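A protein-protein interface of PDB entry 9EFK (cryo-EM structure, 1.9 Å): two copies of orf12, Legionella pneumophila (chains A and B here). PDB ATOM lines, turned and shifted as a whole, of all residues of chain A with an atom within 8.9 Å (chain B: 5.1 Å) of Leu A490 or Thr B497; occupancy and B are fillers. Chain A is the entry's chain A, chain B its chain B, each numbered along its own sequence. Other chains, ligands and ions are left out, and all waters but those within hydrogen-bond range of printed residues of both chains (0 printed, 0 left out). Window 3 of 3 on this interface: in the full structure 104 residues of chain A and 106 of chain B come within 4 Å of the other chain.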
ATOM      1  N   PHE A 483     -14.554  -7.723  17.932  1.00  0.00           N
ATOM      2  CA  PHE A 483     -15.799  -8.297  17.439  1.00  0.00           C
ATOM      3  C   PHE A 483     -16.394  -7.445  16.329  1.00  0.00           C
ATOM      4  O   PHE A 483     -16.870  -7.972  15.320  1.00  0.00           O
ATOM      5  CB  PHE A 483     -16.788  -8.451  18.592  1.00  0.00           C
ATOM      6  CG  PHE A 483     -18.225  -8.520  18.162  1.00  0.00           C
ATOM      7  CD1 PHE A 483     -18.792  -9.722  17.786  1.00  0.00           C
ATOM      8  CD2 PHE A 483     -19.014  -7.384  18.149  1.00  0.00           C
ATOM      9  CE1 PHE A 483     -20.108  -9.786  17.396  1.00  0.00           C
ATOM     10  CE2 PHE A 483     -20.329  -7.446  17.757  1.00  0.00           C
ATOM     11  CZ  PHE A 483     -20.877  -8.647  17.383  1.00  0.00           C
ATOM     12  N   TYR A 484     -16.384  -6.124  16.501  1.00  0.00           N
ATOM     13  CA  TYR A 484     -16.996  -5.253  15.508  1.00  0.00           C
ATOM     14  C   TYR A 484     -16.239  -5.290  14.189  1.00  0.00           C
ATOM     15  O   TYR A 484     -16.853  -5.263  13.120  1.00  0.00           O
ATOM     16  CB  TYR A 484     -17.074  -3.824  16.030  1.00  0.00           C
ATOM     17  CG  TYR A 484     -17.729  -2.879  15.057  1.00  0.00           C
ATOM     18  CD1 TYR A 484     -19.105  -2.732  15.025  1.00  0.00           C
ATOM     19  CD2 TYR A 484     -16.972  -2.135  14.167  1.00  0.00           C
ATOM     20  CE1 TYR A 484     -19.706  -1.873  14.137  1.00  0.00           C
ATOM     21  CE2 TYR A 484     -17.566  -1.279  13.274  1.00  0.00           C
ATOM     22  CZ  TYR A 484     -18.931  -1.150  13.264  1.00  0.00           C
ATOM     23  OH  TYR A 484     -19.525  -0.291  12.375  1.00  0.00           O
ATOM     24  N   GLN A 485     -14.907  -5.329  14.240  1.00  0.00           N
ATOM     25  CA  GLN A 485     -14.135  -5.376  13.004  1.00  0.00           C
ATOM     26  C   GLN A 485     -14.445  -6.638  12.214  1.00  0.00           C
ATOM     27  O   GLN A 485     -14.598  -6.590  10.989  1.00  0.00           O
ATOM     28  CB  GLN A 485     -12.641  -5.288  13.311  1.00  0.00           C
ATOM     29  CG  GLN A 485     -12.206  -3.945  13.852  1.00  0.00           C
ATOM     30  CD  GLN A 485     -10.739  -3.916  14.228  1.00  0.00           C
ATOM     31  OE1 GLN A 485      -9.995  -4.857  13.949  1.00  0.00           O
ATOM     32  NE2 GLN A 485     -10.314  -2.834  14.867  1.00  0.00           N
ATOM     33  N   ALA A 486     -14.543  -7.778  12.897  1.00  0.00           N
ATOM     34  CA  ALA A 486     -14.930  -9.009  12.218  1.00  0.00           C
ATOM     35  C   ALA A 486     -16.360  -8.927  11.702  1.00  0.00           C
ATOM     36  O   ALA A 486     -16.642  -9.350  10.577  1.00  0.00           O
ATOM     37  CB  ALA A 486     -14.765 -10.202  13.157  1.00  0.00           C
ATOM     38  N   ALA A 487     -17.273  -8.386  12.508  1.00  0.00           N
ATOM     39  CA  ALA A 487     -18.669  -8.291  12.095  1.00  0.00           C
ATOM     40  C   ALA A 487     -18.830  -7.365  10.898  1.00  0.00           C
ATOM     41  O   ALA A 487     -19.605  -7.655   9.982  1.00  0.00           O
ATOM     42  CB  ALA A 487     -19.529  -7.816  13.262  1.00  0.00           C
ATOM     43  N   ALA A 488     -18.112  -6.244  10.890  1.00  0.00           N
ATOM     44  CA  ALA A 488     -18.197  -5.314   9.772  1.00  0.00           C
ATOM     45  C   ALA A 488     -17.500  -5.856   8.534  1.00  0.00           C
ATOM     46  O   ALA A 488     -17.833  -5.457   7.415  1.00  0.00           O
ATOM     47  CB  ALA A 488     -17.607  -3.964  10.164  1.00  0.00           C
ATOM     48  N   SER A 489     -16.526  -6.748   8.704  1.00  0.00           N
ATOM     49  CA  SER A 489     -15.886  -7.346   7.540  1.00  0.00           C
ATOM     50  C   SER A 489     -16.809  -8.324   6.832  1.00  0.00           C
ATOM     51  O   SER A 489     -16.739  -8.463   5.608  1.00  0.00           O
ATOM     52  CB  SER A 489     -14.591  -8.043   7.948  1.00  0.00           C
ATOM     53  OG  SER A 489     -13.587  -7.100   8.264  1.00  0.00           O
ATOM     54  N   LEU A 490     -17.678  -9.004   7.576  1.00  0.00           N
ATOM     55  CA  LEU A 490     -18.560 -10.011   7.004  1.00  0.00           C
ATOM     56  C   LEU A 490     -19.880  -9.426   6.521  1.00  0.00           C
ATOM     57  O   LEU A 490     -20.359  -9.792   5.445  1.00  0.00           O
ATOM     58  CB  LEU A 490     -18.831 -11.112   8.029  1.00  0.00           C
ATOM     59  CG  LEU A 490     -17.614 -11.805   8.634  1.00  0.00           C
ATOM     60  CD1 LEU A 490     -18.024 -12.736   9.753  1.00  0.00           C
ATOM     61  CD2 LEU A 490     -16.876 -12.568   7.576  1.00  0.00           C
ATOM     62  N   LEU A 491     -20.480  -8.526   7.294  1.00  0.00           N
ATOM     63  CA  LEU A 491     -21.797  -7.988   6.988  1.00  0.00           C
ATOM     64  C   LEU A 491     -21.773  -6.516   6.618  1.00  0.00           C
ATOM     65  O   LEU A 491     -22.813  -5.969   6.246  1.00  0.00           O
ATOM     66  CB  LEU A 491     -22.734  -8.196   8.179  1.00  0.00           C
ATOM     67  CG  LEU A 491     -22.661  -9.577   8.825  1.00  0.00           C
ATOM     68  CD1 LEU A 491     -23.480  -9.605  10.092  1.00  0.00           C
ATOM     69  CD2 LEU A 491     -23.129 -10.646   7.861  1.00  0.00           C
ATOM     70  N   GLY A 492     -20.625  -5.858   6.717  1.00  0.00           N
ATOM     71  CA  GLY A 492     -20.524  -4.455   6.410  1.00  0.00           C
ATOM     72  C   GLY A 492     -20.978  -3.596   7.568  1.00  0.00           C
ATOM     73  O   GLY A 492     -21.614  -4.072   8.511  1.00  0.00           O
ATOM     74  N   PRO A 493     -20.642  -2.311   7.530  1.00  0.00           N
ATOM     75  CA  PRO A 493     -21.260  -1.362   8.456  1.00  0.00           C
ATOM     76  C   PRO A 493     -22.747  -1.230   8.162  1.00  0.00           C
ATOM     77  O   PRO A 493     -23.258  -1.731   7.158  1.00  0.00           O
ATOM     78  CB  PRO A 493     -20.510  -0.054   8.186  1.00  0.00           C
ATOM     79  CG  PRO A 493     -19.236  -0.473   7.541  1.00  0.00           C
ATOM     80  CD  PRO A 493     -19.567  -1.691   6.741  1.00  0.00           C
ATOM     81  N   ALA A 495     -24.856  -2.799   9.402  1.00  0.00           N
ATOM     82  CA  ALA A 495     -25.346  -4.089   9.862  1.00  0.00           C
ATOM     83  C   ALA A 495     -24.683  -4.528  11.152  1.00  0.00           C
ATOM     84  O   ALA A 495     -25.364  -4.998  12.062  1.00  0.00           O
ATOM     85  CB  ALA A 495     -25.127  -5.160   8.792  1.00  0.00           C
ATOM     86  N   ALA A 496     -23.361  -4.384  11.241  1.00  0.00           N
ATOM     87  CA  ALA A 496     -22.677  -4.603  12.508  1.00  0.00           C
ATOM     88  C   ALA A 496     -23.115  -3.580  13.545  1.00  0.00           C
ATOM     89  O   ALA A 496     -23.311  -3.919  14.716  1.00  0.00           O
ATOM     90  CB  ALA A 496     -21.166  -4.554  12.298  1.00  0.00           C
ATOM     91  N   LEU B 480     -13.287 -18.105   9.873  1.00  0.00           N
ATOM     92  CA  LEU B 480     -14.463 -17.488   9.271  1.00  0.00           C
ATOM     93  C   LEU B 480     -14.083 -16.307   8.386  1.00  0.00           C
ATOM     94  O   LEU B 480     -14.640 -16.139   7.298  1.00  0.00           O
ATOM     95  CB  LEU B 480     -15.433 -17.060  10.369  1.00  0.00           C
ATOM     96  CG  LEU B 480     -16.701 -16.305   9.983  1.00  0.00           C
ATOM     97  CD1 LEU B 480     -17.407 -16.977   8.834  1.00  0.00           C
ATOM     98  CD2 LEU B 480     -17.619 -16.217  11.183  1.00  0.00           C
ATOM     99  N   LEU B 481     -13.138 -15.481   8.833  1.00  0.00           N
ATOM    100  CA  LEU B 481     -12.706 -14.348   8.022  1.00  0.00           C
ATOM    101  C   LEU B 481     -11.943 -14.809   6.788  1.00  0.00           C
ATOM    102  O   LEU B 481     -12.072 -14.212   5.713  1.00  0.00           O
ATOM    103  CB  LEU B 481     -11.851 -13.401   8.857  1.00  0.00           C
ATOM    104  CG  LEU B 481     -12.564 -12.666   9.988  1.00  0.00           C
ATOM    105  CD1 LEU B 481     -11.595 -11.764  10.721  1.00  0.00           C
ATOM    106  CD2 LEU B 481     -13.729 -11.866   9.445  1.00  0.00           C
ATOM    107  N   TYR B 484     -14.454 -15.848   4.195  1.00  0.00           N
ATOM    108  CA  TYR B 484     -15.135 -14.744   3.529  1.00  0.00           C
ATOM    109  C   TYR B 484     -14.232 -14.065   2.511  1.00  0.00           C
ATOM    110  O   TYR B 484     -14.694 -13.672   1.436  1.00  0.00           O
ATOM    111  CB  TYR B 484     -15.631 -13.733   4.555  1.00  0.00           C
ATOM    112  CG  TYR B 484     -16.404 -12.598   3.936  1.00  0.00           C
ATOM    113  CD1 TYR B 484     -17.749 -12.734   3.640  1.00  0.00           C
ATOM    114  CD2 TYR B 484     -15.787 -11.394   3.640  1.00  0.00           C
ATOM    115  CE1 TYR B 484     -18.457 -11.702   3.071  1.00  0.00           C
ATOM    116  CE2 TYR B 484     -16.486 -10.360   3.070  1.00  0.00           C
ATOM    117  CZ  TYR B 484     -17.819 -10.519   2.788  1.00  0.00           C
ATOM    118  OH  TYR B 484     -18.518  -9.486   2.218  1.00  0.00           O
ATOM    119  N   GLU B 494     -21.626  -8.768  -1.655  1.00  0.00           N
ATOM    120  CA  GLU B 494     -23.063  -8.807  -1.924  1.00  0.00           C
ATOM    121  C   GLU B 494     -23.477 -10.206  -2.361  1.00  0.00           C
ATOM    122  O   GLU B 494     -24.670 -10.519  -2.420  1.00  0.00           O
ATOM    123  CB  GLU B 494     -23.472  -7.751  -2.966  1.00  0.00           C
ATOM    124  CG  GLU B 494     -23.870  -8.293  -4.337  1.00  0.00           C
ATOM    125  CD  GLU B 494     -25.378  -8.399  -4.524  1.00  0.00           C
ATOM    126  OE1 GLU B 494     -26.090  -7.419  -4.219  1.00  0.00           O
ATOM    127  OE2 GLU B 494     -25.854  -9.462  -4.975  1.00  0.00           O
ATOM    128  N   ALA B 495     -22.501 -11.066  -2.619  1.00  0.00           N
ATOM    129  CA  ALA B 495     -22.728 -12.480  -2.880  1.00  0.00           C
ATOM    130  C   ALA B 495     -22.148 -13.368  -1.796  1.00  0.00           C
ATOM    131  O   ALA B 495     -22.796 -14.326  -1.378  1.00  0.00           O
ATOM    132  CB  ALA B 495     -22.131 -12.875  -4.232  1.00  0.00           C
ATOM    133  N   ALA B 496     -20.933 -13.068  -1.339  1.00  0.00           N
ATOM    134  CA  ALA B 496     -20.392 -13.745  -0.169  1.00  0.00           C
ATOM    135  C   ALA B 496     -21.198 -13.406   1.077  1.00  0.00           C
ATOM    136  O   ALA B 496     -21.465 -14.283   1.905  1.00  0.00           O
ATOM    137  CB  ALA B 496     -18.923 -13.375   0.018  1.00  0.00           C
ATOM    138  N   THR B 497     -21.589 -12.138   1.229  1.00  0.00           N
ATOM    139  CA  THR B 497     -22.432 -11.749   2.355  1.00  0.00           C
ATOM    140  C   THR B 497     -23.816 -12.378   2.253  1.00  0.00           C
ATOM    141  O   THR B 497     -24.393 -12.791   3.265  1.00  0.00           O
ATOM    142  CB  THR B 497     -22.542 -10.227   2.435  1.00  0.00           C
ATOM    143  OG1 THR B 497     -21.243  -9.663   2.639  1.00  0.00           O
ATOM    144  CG2 THR B 497     -23.437  -9.815   3.586  1.00  0.00           C
ATOM    145  N   ALA B 498     -24.365 -12.457   1.040  1.00  0.00           N
ATOM    146  CA  ALA B 498     -25.685 -13.050   0.866  1.00  0.00           C
ATOM    147  C   ALA B 498     -25.692 -14.527   1.230  1.00  0.00           C
ATOM    148  O   ALA B 498     -26.714 -15.049   1.685  1.00  0.00           O
ATOM    149  CB  ALA B 498     -26.162 -12.855  -0.570  1.00  0.00           C
ATOM    150  N   SER B 499     -24.570 -15.217   1.045  1.00  0.00           N
ATOM    151  CA  SER B 499     -24.472 -16.640   1.361  1.00  0.00           C
ATOM    152  C   SER B 499     -24.035 -16.866   2.803  1.00  0.00           C
ATOM    153  O   SER B 499     -23.141 -17.656   3.089  1.00  0.00           O
ATOM    154  CB  SER B 499     -23.508 -17.314   0.395  1.00  0.00           C
ATOM    155  OG  SER B 499     -22.179 -16.895   0.638  1.00  0.00           O
ATOM    156  N   LEU B 500     -24.687 -16.178   3.729  1.00  0.00           N
ATOM    157  CA  LEU B 500     -24.340 -16.241   5.137  1.00  0.00           C
ATOM    158  C   LEU B 500     -25.622 -16.248   5.948  1.00  0.00           C
ATOM    159  O   LEU B 500     -26.642 -15.703   5.522  1.00  0.00           O
ATOM    160  CB  LEU B 500     -23.465 -15.052   5.552  1.00  0.00           C
ATOM    161  CG  LEU B 500     -22.043 -15.266   6.069  1.00  0.00           C
ATOM    162  CD1 LEU B 500     -21.202 -16.041   5.084  1.00  0.00           C
ATOM    163  CD2 LEU B 500     -21.401 -13.925   6.353  1.00  0.00           C
ATOM    164  N   VAL B 505     -24.081 -15.841  12.423  1.00  0.00           N
ATOM    165  CA  VAL B 505     -22.742 -15.264  12.358  1.00  0.00           C
ATOM    166  C   VAL B 505     -22.527 -14.286  13.507  1.00  0.00           C
ATOM    167  O   VAL B 505     -21.490 -14.310  14.178  1.00  0.00           O
ATOM    168  CB  VAL B 505     -22.516 -14.590  10.994  1.00  0.00           C
ATOM    169  CG1 VAL B 505     -21.296 -13.698  11.041  1.00  0.00           C
ATOM    170  CG2 VAL B 505     -22.361 -15.636   9.910  1.00  0.00           C
ATOM    171  N   LEU B 509     -19.836 -14.934  16.431  1.00  0.00           N
ATOM    172  CA  LEU B 509     -18.730 -13.995  16.571  1.00  0.00           C
ATOM    173  C   LEU B 509     -18.643 -13.466  17.995  1.00  0.00           C
ATOM    174  O   LEU B 509     -17.547 -13.320  18.545  1.00  0.00           O
ATOM    175  CB  LEU B 509     -18.883 -12.841  15.585  1.00  0.00           C
ATOM    176  CG  LEU B 509     -18.447 -13.080  14.144  1.00  0.00           C
ATOM    177  CD1 LEU B 509     -18.597 -11.803  13.354  1.00  0.00           C
ATOM    178  CD2 LEU B 509     -17.018 -13.573  14.090  1.00  0.00           C
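Positions printed for both chains: 484, 495 and 496.
Among the printed residues, pairs that only touch across the chains: Phe A483 with Leu B509 (3.8 Å), Ala A487 with Leu B509 (3.7 Å), Ser A489 with Tyr B484 (3.2 Å), Leu A490 with Leu B480 (3.8 Å), Leu A490 with Leu B481 (3.7 Å), Leu A490 with Tyr B484 (3.5 Å), Leu A490 with Val B505 (3.6 Å) and Leu A490 with Leu B509 (3.8 Å).
The backbone carbonyl oxygen of Gln A485 lies within hydrogen-bond range of the side-chain hydroxyl of Ser A489 (3.0 Å). The side-chain hydroxyl of Tyr B484 is in hydrogen-bond range of the side-chain hydroxyl of Thr B497, 2.8 Å away.
Hydrophobic or aromatic side chains of chain A that line the printed part of chain B: Phe A483 and Leu A490. Printed residues of chain B that touch a printed residue of chain A: Leu B480, Leu B481, Tyr B484, Thr B497, Val B505 and Leu B509. Among the printed residues, 9 pairs touch across the chains. Among the printed residues, no Asp or Glu carboxylate lies within 4 Å of a Lys or Arg side-chain nitrogen of the other chain.
O of Leu A490 is in hydrogen-bond range of OG1 of Thr B497.
Of the printed residues of chain B, Leu A490 touches Leu B480 (3.8 Å), Leu B481 (3.7 Å), Tyr B484 (3.5 Å), Thr B497 (2.9 Å), Val B505 (3.6 Å) and Leu B509 (3.8 Å). Thr B497 touches just one residue of chain A: Leu A490 (2.9 Å). No residue of chain A comes within 4 Å of Ala B496. No residue of chain A comes within 4 Å of Ala B498. Of the printed residues of chain A, Leu B481 touches Leu A490. Printed residues of chain A within 4 Å of Val B505: Leu A490. Of the printed residues of chain A, Leu B509 touches Phe A483, Ala A487 and Leu A490. Of the printed residues of chain A, Leu B480 touches Leu A490. Printed residues of chain B within 4 Å of Ser A489: Tyr B484. Ala A486 touches none of the printed residues of chain B. The nearest residue of chain A that does not touch Thr B497 is Leu A491 (4.2 Å).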
